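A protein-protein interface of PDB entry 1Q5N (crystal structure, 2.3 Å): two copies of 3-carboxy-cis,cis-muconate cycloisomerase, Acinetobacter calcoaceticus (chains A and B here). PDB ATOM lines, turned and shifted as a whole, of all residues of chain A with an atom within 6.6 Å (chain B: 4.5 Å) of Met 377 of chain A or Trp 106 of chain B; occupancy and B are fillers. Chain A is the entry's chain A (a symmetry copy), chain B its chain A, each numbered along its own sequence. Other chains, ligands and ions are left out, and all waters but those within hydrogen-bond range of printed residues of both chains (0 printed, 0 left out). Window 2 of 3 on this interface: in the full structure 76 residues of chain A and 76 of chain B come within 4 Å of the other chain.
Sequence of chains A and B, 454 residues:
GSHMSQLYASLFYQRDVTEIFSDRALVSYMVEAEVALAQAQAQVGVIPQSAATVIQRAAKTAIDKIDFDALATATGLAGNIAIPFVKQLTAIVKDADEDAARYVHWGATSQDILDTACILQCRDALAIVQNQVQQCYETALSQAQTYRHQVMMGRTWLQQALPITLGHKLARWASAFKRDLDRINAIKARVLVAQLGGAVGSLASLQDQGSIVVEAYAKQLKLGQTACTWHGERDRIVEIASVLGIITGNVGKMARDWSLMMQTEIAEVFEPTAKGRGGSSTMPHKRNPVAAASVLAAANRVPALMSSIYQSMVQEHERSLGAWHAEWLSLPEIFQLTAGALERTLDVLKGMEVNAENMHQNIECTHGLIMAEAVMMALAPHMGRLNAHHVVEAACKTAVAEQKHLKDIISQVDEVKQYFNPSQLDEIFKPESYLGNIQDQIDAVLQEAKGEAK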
ATOM      1  N   ALA A 372      15.583  -7.267   6.103  1.00  0.00           N
ATOM      2  CA  ALA A 372      16.825  -7.943   5.752  1.00  0.00           C
ATOM      3  C   ALA A 372      16.961  -8.264   4.278  1.00  0.00           C
ATOM      4  O   ALA A 372      18.035  -8.085   3.679  1.00  0.00           O
ATOM      5  CB  ALA A 372      16.974  -9.223   6.559  1.00  0.00           C
ATOM      6  N   GLU A 373      15.903  -8.762   3.670  1.00  0.00           N
ATOM      7  CA  GLU A 373      16.057  -9.101   2.272  1.00  0.00           C
ATOM      8  C   GLU A 373      16.128  -7.839   1.377  1.00  0.00           C
ATOM      9  O   GLU A 373      16.849  -7.844   0.390  1.00  0.00           O
ATOM     10  CB  GLU A 373      15.017 -10.159   1.857  1.00  0.00           C
ATOM     11  CG  GLU A 373      13.852  -9.740   1.076  1.00  0.00           C
ATOM     12  CD  GLU A 373      13.158 -10.957   0.463  1.00  0.00           C
ATOM     13  OE1 GLU A 373      13.103 -11.993   1.172  1.00  0.00           O
ATOM     14  OE2 GLU A 373      12.660 -10.887  -0.686  1.00  0.00           O
ATOM     15  N   ALA A 374      15.461  -6.758   1.773  1.00  0.00           N
ATOM     16  CA  ALA A 374      15.543  -5.506   1.045  1.00  0.00           C
ATOM     17  C   ALA A 374      17.045  -5.039   1.083  1.00  0.00           C
ATOM     18  O   ALA A 374      17.602  -4.636   0.048  1.00  0.00           O
ATOM     19  CB  ALA A 374      14.625  -4.437   1.709  1.00  0.00           C
ATOM     20  N   VAL A 375      17.698  -5.113   2.251  1.00  0.00           N
ATOM     21  CA  VAL A 375      19.112  -4.705   2.356  1.00  0.00           C
ATOM     22  C   VAL A 375      20.007  -5.571   1.457  1.00  0.00           C
ATOM     23  O   VAL A 375      20.952  -5.103   0.820  1.00  0.00           O
ATOM     24  CB  VAL A 375      19.640  -4.819   3.814  1.00  0.00           C
ATOM     25  CG1 VAL A 375      21.124  -4.454   3.858  1.00  0.00           C
ATOM     26  CG2 VAL A 375      18.830  -3.907   4.738  1.00  0.00           C
ATOM     27  N   MET A 376      19.690  -6.849   1.414  1.00  0.00           N
ATOM     28  CA  MET A 376      20.428  -7.771   0.607  1.00  0.00           C
ATOM     29  C   MET A 376      20.303  -7.471  -0.915  1.00  0.00           C
ATOM     30  O   MET A 376      21.286  -7.600  -1.649  1.00  0.00           O
ATOM     31  CB  MET A 376      19.939  -9.161   0.952  1.00  0.00           C
ATOM     32  CG  MET A 376      20.930 -10.227   0.672  1.00  0.00           C
ATOM     33  SD  MET A 376      20.049 -11.414  -0.279  1.00  0.00           S
ATOM     34  CE  MET A 376      20.308 -10.678  -1.979  1.00  0.00           C
ATOM     35  N   MET A 377      19.102  -7.078  -1.371  1.00  0.00           N
ATOM     36  CA  MET A 377      18.871  -6.718  -2.795  1.00  0.00           C
ATOM     37  C   MET A 377      19.635  -5.433  -3.169  1.00  0.00           C
ATOM     38  O   MET A 377      20.162  -5.330  -4.270  1.00  0.00           O
ATOM     39  CB  MET A 377      17.382  -6.473  -3.081  1.00  0.00           C
ATOM     40  CG  MET A 377      16.496  -7.681  -2.944  1.00  0.00           C
ATOM     41  SD  MET A 377      16.835  -8.911  -4.191  1.00  0.00           S
ATOM     42  CE  MET A 377      17.497 -10.238  -3.199  1.00  0.00           C
ATOM     43  N   ALA A 378      19.660  -4.453  -2.265  1.00  0.00           N
ATOM     44  CA  ALA A 378      20.382  -3.200  -2.503  1.00  0.00           C
ATOM     45  C   ALA A 378      21.883  -3.440  -2.610  1.00  0.00           C
ATOM     46  O   ALA A 378      22.559  -2.733  -3.350  1.00  0.00           O
ATOM     47  CB  ALA A 378      20.113  -2.214  -1.382  1.00  0.00           C
ATOM     48  N   LEU A 379      22.398  -4.435  -1.876  1.00  0.00           N
ATOM     49  CA  LEU A 379      23.826  -4.762  -1.877  1.00  0.00           C
ATOM     50  C   LEU A 379      24.286  -5.688  -2.985  1.00  0.00           C
ATOM     51  O   LEU A 379      25.450  -5.633  -3.367  1.00  0.00           O
ATOM     52  CB  LEU A 379      24.248  -5.414  -0.556  1.00  0.00           C
ATOM     53  CG  LEU A 379      24.703  -4.528   0.598  1.00  0.00           C
ATOM     54  CD1 LEU A 379      26.121  -4.016   0.391  1.00  0.00           C
ATOM     55  CD2 LEU A 379      23.765  -3.357   0.689  1.00  0.00           C
ATOM     56  N   ALA A 380      23.388  -6.551  -3.465  1.00  0.00           N
ATOM     57  CA  ALA A 380      23.700  -7.556  -4.497  1.00  0.00           C
ATOM     58  C   ALA A 380      24.513  -7.033  -5.687  1.00  0.00           C
ATOM     59  O   ALA A 380      25.512  -7.650  -6.069  1.00  0.00           O
ATOM     60  CB  ALA A 380      22.417  -8.224  -4.999  1.00  0.00           C
ATOM     61  N   PRO A 381      24.097  -5.893  -6.282  1.00  0.00           N
ATOM     62  CA  PRO A 381      24.791  -5.293  -7.430  1.00  0.00           C
ATOM     63  C   PRO A 381      26.269  -4.928  -7.141  1.00  0.00           C
ATOM     64  O   PRO A 381      27.171  -5.258  -7.913  1.00  0.00           O
ATOM     65  CB  PRO A 381      23.944  -4.049  -7.732  1.00  0.00           C
ATOM     66  CG  PRO A 381      22.579  -4.431  -7.244  1.00  0.00           C
ATOM     67  CD  PRO A 381      22.893  -5.111  -5.944  1.00  0.00           C
ATOM     68  N   ARG A 385      25.322 -11.508  -5.159  1.00  0.00           N
ATOM     69  CA  ARG A 385      24.323 -11.990  -4.213  1.00  0.00           C
ATOM     70  C   ARG A 385      24.856 -12.852  -3.057  1.00  0.00           C
ATOM     71  O   ARG A 385      24.347 -12.772  -1.946  1.00  0.00           O
ATOM     72  CB  ARG A 385      23.202 -12.741  -4.943  1.00  0.00           C
ATOM     73  CG  ARG A 385      21.793 -12.427  -4.383  1.00  0.00           C
ATOM     74  CD  ARG A 385      20.767 -13.530  -4.690  1.00  0.00           C
ATOM     75  NE  ARG A 385      20.274 -13.518  -6.079  1.00  0.00           N
ATOM     76  CZ  ARG A 385      19.876 -14.601  -6.762  1.00  0.00           C
ATOM     77  NH1 ARG A 385      19.916 -15.803  -6.186  1.00  0.00           N
ATOM     78  NH2 ARG A 385      19.432 -14.487  -8.023  1.00  0.00           N
ATOM     79  N   ALA A 388      26.458 -10.511  -0.596  1.00  0.00           N
ATOM     80  CA  ALA A 388      25.425  -9.693   0.016  1.00  0.00           C
ATOM     81  C   ALA A 388      24.702 -10.551   1.060  1.00  0.00           C
ATOM     82  O   ALA A 388      24.516 -10.138   2.194  1.00  0.00           O
ATOM     83  CB  ALA A 388      24.448  -9.191  -1.045  1.00  0.00           C
ATOM     84  N   VAL A 392      24.619  -9.724   5.339  1.00  0.00           N
ATOM     85  CA  VAL A 392      23.350  -9.460   5.978  1.00  0.00           C
ATOM     86  C   VAL A 392      23.028 -10.496   7.052  1.00  0.00           C
ATOM     87  O   VAL A 392      22.570 -10.149   8.136  1.00  0.00           O
ATOM     88  CB  VAL A 392      22.223  -9.330   4.914  1.00  0.00           C
ATOM     89  CG1 VAL A 392      20.867  -9.162   5.582  1.00  0.00           C
ATOM     90  CG2 VAL A 392      22.498  -8.101   4.053  1.00  0.00           C
ATOM     91  N   TYR A 434      10.077  -1.144  -0.325  1.00  0.00           N
ATOM     92  CA  TYR A 434      10.088  -2.551  -0.698  1.00  0.00           C
ATOM     93  C   TYR A 434       8.678  -3.121  -0.888  1.00  0.00           C
ATOM     94  O   TYR A 434       8.308  -4.103  -0.234  1.00  0.00           O
ATOM     95  CB  TYR A 434      10.855  -3.339   0.377  1.00  0.00           C
ATOM     96  CG  TYR A 434      11.390  -4.628  -0.154  1.00  0.00           C
ATOM     97  CD1 TYR A 434      12.236  -4.622  -1.247  1.00  0.00           C
ATOM     98  CD2 TYR A 434      11.109  -5.840   0.468  1.00  0.00           C
ATOM     99  CE1 TYR A 434      12.800  -5.770  -1.707  1.00  0.00           C
ATOM    100  CE2 TYR A 434      11.668  -6.997   0.023  1.00  0.00           C
ATOM    101  CZ  TYR A 434      12.521  -6.957  -1.072  1.00  0.00           C
ATOM    102  OH  TYR A 434      13.107  -8.091  -1.572  1.00  0.00           O
ATOM    103  N   LEU B  37       8.910 -20.116 -15.200  1.00  0.00           N
ATOM    104  CA  LEU B  37       9.343 -18.945 -14.441  1.00  0.00           C
ATOM    105  C   LEU B  37      10.733 -18.434 -14.908  1.00  0.00           C
ATOM    106  O   LEU B  37      10.930 -17.231 -15.064  1.00  0.00           O
ATOM    107  CB  LEU B  37       9.407 -19.279 -12.940  1.00  0.00           C
ATOM    108  CG  LEU B  37       9.864 -18.094 -12.069  1.00  0.00           C
ATOM    109  CD1 LEU B  37       8.869 -16.971 -12.196  1.00  0.00           C
ATOM    110  CD2 LEU B  37       9.999 -18.514 -10.623  1.00  0.00           C
ATOM    111  N   GLN B  41      11.432 -14.994 -17.049  1.00  0.00           N
ATOM    112  CA  GLN B  41      12.370 -14.012 -16.511  1.00  0.00           C
ATOM    113  C   GLN B  41      13.525 -13.713 -17.483  1.00  0.00           C
ATOM    114  O   GLN B  41      13.922 -12.556 -17.625  1.00  0.00           O
ATOM    115  CB  GLN B  41      12.917 -14.467 -15.152  1.00  0.00           C
ATOM    116  CG  GLN B  41      11.874 -14.419 -14.092  1.00  0.00           C
ATOM    117  CD  GLN B  41      12.339 -14.983 -12.759  1.00  0.00           C
ATOM    118  OE1 GLN B  41      13.237 -15.830 -12.700  1.00  0.00           O
ATOM    119  NE2 GLN B  41      11.703 -14.529 -11.672  1.00  0.00           N
ATOM    120  N   VAL B  46      15.182 -10.182 -16.450  1.00  0.00           N
ATOM    121  CA  VAL B  46      15.460 -10.435 -15.036  1.00  0.00           C
ATOM    122  C   VAL B  46      16.557 -11.477 -14.744  1.00  0.00           C
ATOM    123  O   VAL B  46      17.209 -11.398 -13.713  1.00  0.00           O
ATOM    124  CB  VAL B  46      14.167 -10.786 -14.289  1.00  0.00           C
ATOM    125  CG1 VAL B  46      14.453 -11.049 -12.804  1.00  0.00           C
ATOM    126  CG2 VAL B  46      13.174  -9.639 -14.473  1.00  0.00           C
ATOM    127  N   ILE B  47      16.748 -12.481 -15.589  1.00  0.00           N
ATOM    128  CA  ILE B  47      17.861 -13.396 -15.335  1.00  0.00           C
ATOM    129  C   ILE B  47      18.470 -13.680 -16.697  1.00  0.00           C
ATOM    130  O   ILE B  47      17.804 -13.531 -17.731  1.00  0.00           O
ATOM    131  CB  ILE B  47      17.473 -14.748 -14.660  1.00  0.00           C
ATOM    132  CG1 ILE B  47      16.671 -15.608 -15.634  1.00  0.00           C
ATOM    133  CG2 ILE B  47      16.777 -14.486 -13.324  1.00  0.00           C
ATOM    134  CD1 ILE B  47      16.461 -17.009 -15.170  1.00  0.00           C
ATOM    135  N   TYR B 103      19.577 -18.995 -10.038  1.00  0.00           N
ATOM    136  CA  TYR B 103      18.354 -18.448 -10.555  1.00  0.00           C
ATOM    137  C   TYR B 103      17.138 -19.378 -10.454  1.00  0.00           C
ATOM    138  O   TYR B 103      16.058 -19.028 -10.935  1.00  0.00           O
ATOM    139  CB  TYR B 103      18.595 -18.007 -11.996  1.00  0.00           C
ATOM    140  CG  TYR B 103      19.701 -16.990 -12.063  1.00  0.00           C
ATOM    141  CD1 TYR B 103      19.476 -15.662 -11.682  1.00  0.00           C
ATOM    142  CD2 TYR B 103      20.991 -17.359 -12.463  1.00  0.00           C
ATOM    143  CE1 TYR B 103      20.491 -14.739 -11.694  1.00  0.00           C
ATOM    144  CE2 TYR B 103      22.016 -16.442 -12.479  1.00  0.00           C
ATOM    145  CZ  TYR B 103      21.764 -15.133 -12.094  1.00  0.00           C
ATOM    146  OH  TYR B 103      22.790 -14.214 -12.103  1.00  0.00           O
ATOM    147  N   VAL B 104      17.307 -20.551  -9.843  1.00  0.00           N
ATOM    148  CA  VAL B 104      16.174 -21.466  -9.684  1.00  0.00           C
ATOM    149  C   VAL B 104      15.217 -20.886  -8.631  1.00  0.00           C
ATOM    150  O   VAL B 104      15.658 -20.516  -7.531  1.00  0.00           O
ATOM    151  CB  VAL B 104      16.621 -22.859  -9.191  1.00  0.00           C
ATOM    152  CG1 VAL B 104      15.405 -23.762  -8.929  1.00  0.00           C
ATOM    153  CG2 VAL B 104      17.527 -23.490 -10.217  1.00  0.00           C
ATOM    154  N   HIS B 105      13.935 -20.766  -8.992  1.00  0.00           N
ATOM    155  CA  HIS B 105      12.913 -20.298  -8.063  1.00  0.00           C
ATOM    156  C   HIS B 105      13.141 -18.843  -7.690  1.00  0.00           C
ATOM    157  O   HIS B 105      12.811 -18.425  -6.581  1.00  0.00           O
ATOM    158  CB  HIS B 105      12.953 -21.173  -6.793  1.00  0.00           C
ATOM    159  CG  HIS B 105      11.768 -21.004  -5.891  1.00  0.00           C
ATOM    160  ND1 HIS B 105      10.511 -21.477  -6.213  1.00  0.00           N
ATOM    161  CD2 HIS B 105      11.662 -20.472  -4.647  1.00  0.00           C
ATOM    162  CE1 HIS B 105       9.685 -21.248  -5.208  1.00  0.00           C
ATOM    163  NE2 HIS B 105      10.354 -20.639  -4.244  1.00  0.00           N
ATOM    164  N   TRP B 106      13.713 -18.089  -8.629  1.00  0.00           N
ATOM    165  CA  TRP B 106      14.036 -16.679  -8.412  1.00  0.00           C
ATOM    166  C   TRP B 106      12.811 -15.813  -8.197  1.00  0.00           C
ATOM    167  O   TRP B 106      12.003 -15.677  -9.100  1.00  0.00           O
ATOM    168  CB  TRP B 106      14.826 -16.114  -9.616  1.00  0.00           C
ATOM    169  CG  TRP B 106      15.163 -14.674  -9.423  1.00  0.00           C
ATOM    170  CD1 TRP B 106      14.781 -13.618 -10.212  1.00  0.00           C
ATOM    171  CD2 TRP B 106      15.822 -14.108  -8.287  1.00  0.00           C
ATOM    172  NE1 TRP B 106      15.157 -12.427  -9.628  1.00  0.00           N
ATOM    173  CE2 TRP B 106      15.798 -12.697  -8.444  1.00  0.00           C
ATOM    174  CE3 TRP B 106      16.429 -14.659  -7.140  1.00  0.00           C
ATOM    175  CZ2 TRP B 106      16.353 -11.816  -7.489  1.00  0.00           C
ATOM    176  CZ3 TRP B 106      16.987 -13.789  -6.175  1.00  0.00           C
ATOM    177  CH2 TRP B 106      16.944 -12.376  -6.362  1.00  0.00           C
ATOM    178  N   GLY B 107      12.681 -15.217  -7.019  1.00  0.00           N
ATOM    179  CA  GLY B 107      11.533 -14.349  -6.758  1.00  0.00           C
ATOM    180  C   GLY B 107      10.157 -14.952  -6.400  1.00  0.00           C
ATOM    181  O   GLY B 107       9.246 -14.226  -6.034  1.00  0.00           O
ATOM    182  N   ALA B 108       9.988 -16.266  -6.489  1.00  0.00           N
ATOM    183  CA  ALA B 108       8.710 -16.879  -6.172  1.00  0.00           C
ATOM    184  C   ALA B 108       8.645 -17.329  -4.727  1.00  0.00           C
ATOM    185  O   ALA B 108       9.668 -17.408  -4.023  1.00  0.00           O
ATOM    186  CB  ALA B 108       8.473 -18.074  -7.072  1.00  0.00           C
ATOM    187  N   SER B 205      10.798  -8.843  -4.257  1.00  0.00           N
ATOM    188  CA  SER B 205      12.153  -9.120  -4.728  1.00  0.00           C
ATOM    189  C   SER B 205      12.398  -8.907  -6.252  1.00  0.00           C
ATOM    190  O   SER B 205      13.557  -8.941  -6.712  1.00  0.00           O
ATOM    191  CB  SER B 205      12.593 -10.538  -4.325  1.00  0.00           C
ATOM    192  OG  SER B 205      11.793 -11.494  -4.974  1.00  0.00           O
ATOM    193  N   LEU B 206      11.332  -8.692  -7.023  1.00  0.00           N
ATOM    194  CA  LEU B 206      11.474  -8.426  -8.450  1.00  0.00           C
ATOM    195  C   LEU B 206      11.414  -6.910  -8.697  1.00  0.00           C
ATOM    196  O   LEU B 206      11.441  -6.457  -9.837  1.00  0.00           O
ATOM    197  CB  LEU B 206      10.360  -9.135  -9.240  1.00  0.00           C
ATOM    198  CG  LEU B 206      10.479 -10.666  -9.290  1.00  0.00           C
ATOM    199  CD1 LEU B 206       9.353 -11.242 -10.110  1.00  0.00           C
ATOM    200  CD2 LEU B 206      11.815 -11.067  -9.894  1.00  0.00           C
ATOM    201  N   GLN B 207      11.271  -6.146  -7.616  1.00  0.00           N
ATOM    202  CA  GLN B 207      11.221  -4.688  -7.651  1.00  0.00           C
ATOM    203  C   GLN B 207      10.272  -3.961  -8.588  1.00  0.00           C
ATOM    204  O   GLN B 207       9.121  -3.762  -8.244  1.00  0.00           O
ATOM    205  CB  GLN B 207      12.658  -4.183  -7.793  1.00  0.00           C
ATOM    206  CG  GLN B 207      13.388  -4.576  -6.488  1.00  0.00           C
ATOM    207  CD  GLN B 207      14.887  -4.443  -6.493  1.00  0.00           C
ATOM    208  OE1 GLN B 207      15.590  -5.084  -7.299  1.00  0.00           O
ATOM    209  NE2 GLN B 207      15.402  -3.629  -5.561  1.00  0.00           N
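Printed residues of chain B that touch a printed residue of chain A: Tyr 103, Trp 106 and Ser 205.
Hydrophobic or aromatic side chains of chain B within 4 Å of the printed part of chain A: Tyr 103 and Trp 106.
Of the 14 printed residues of chain A, 4 touch a printed residue of chain B.
No position is printed for both chains.
Of the printed residues of chain B, Glu 373 of chain A touches Ser 205 (3.7 Å).
Met 377 of chain A touches just one residue of chain B: Trp 106.
Of the printed residues of chain A, Trp 106 of chain B touches Met 377 (3.9 Å) and Arg 385 (3.1 Å).
Printed residues of chain A within 4 Å of Ser 205 of chain B: Glu 373 (3.7 Å) and Tyr 434 (3.5 Å).
The nearest printed residue of chain B that does not touch Glu 373 of chain A is Leu 206 of chain B (6.8 Å).
Among the printed residues, pairs that only touch across the chains: Arg 385 of chain A with Trp 106 of chain B (3.1 Å), Tyr 434 of chain A with Ser 205 of chain B (3.5 Å), Glu 373 of chain A with Ser 205 of chain B (3.7 Å), Arg 385 of chain A with Tyr 103 of chain B (3.8 Å) and Met 377 of chain A with Trp 106 of chain B (3.9 Å).
The side-chain amide nitrogen of Gln 41 of chain B is in hydrogen-bond range of the backbone carbonyl oxygen of Trp 106 of chain B, 2.8 Å away.
The side-chain carboxylate (OE2) of Glu 373 of chain A lies within hydrogen-bond range of the side-chain hydroxyl (OH) of Tyr 434 of chain A (3.0 Å).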
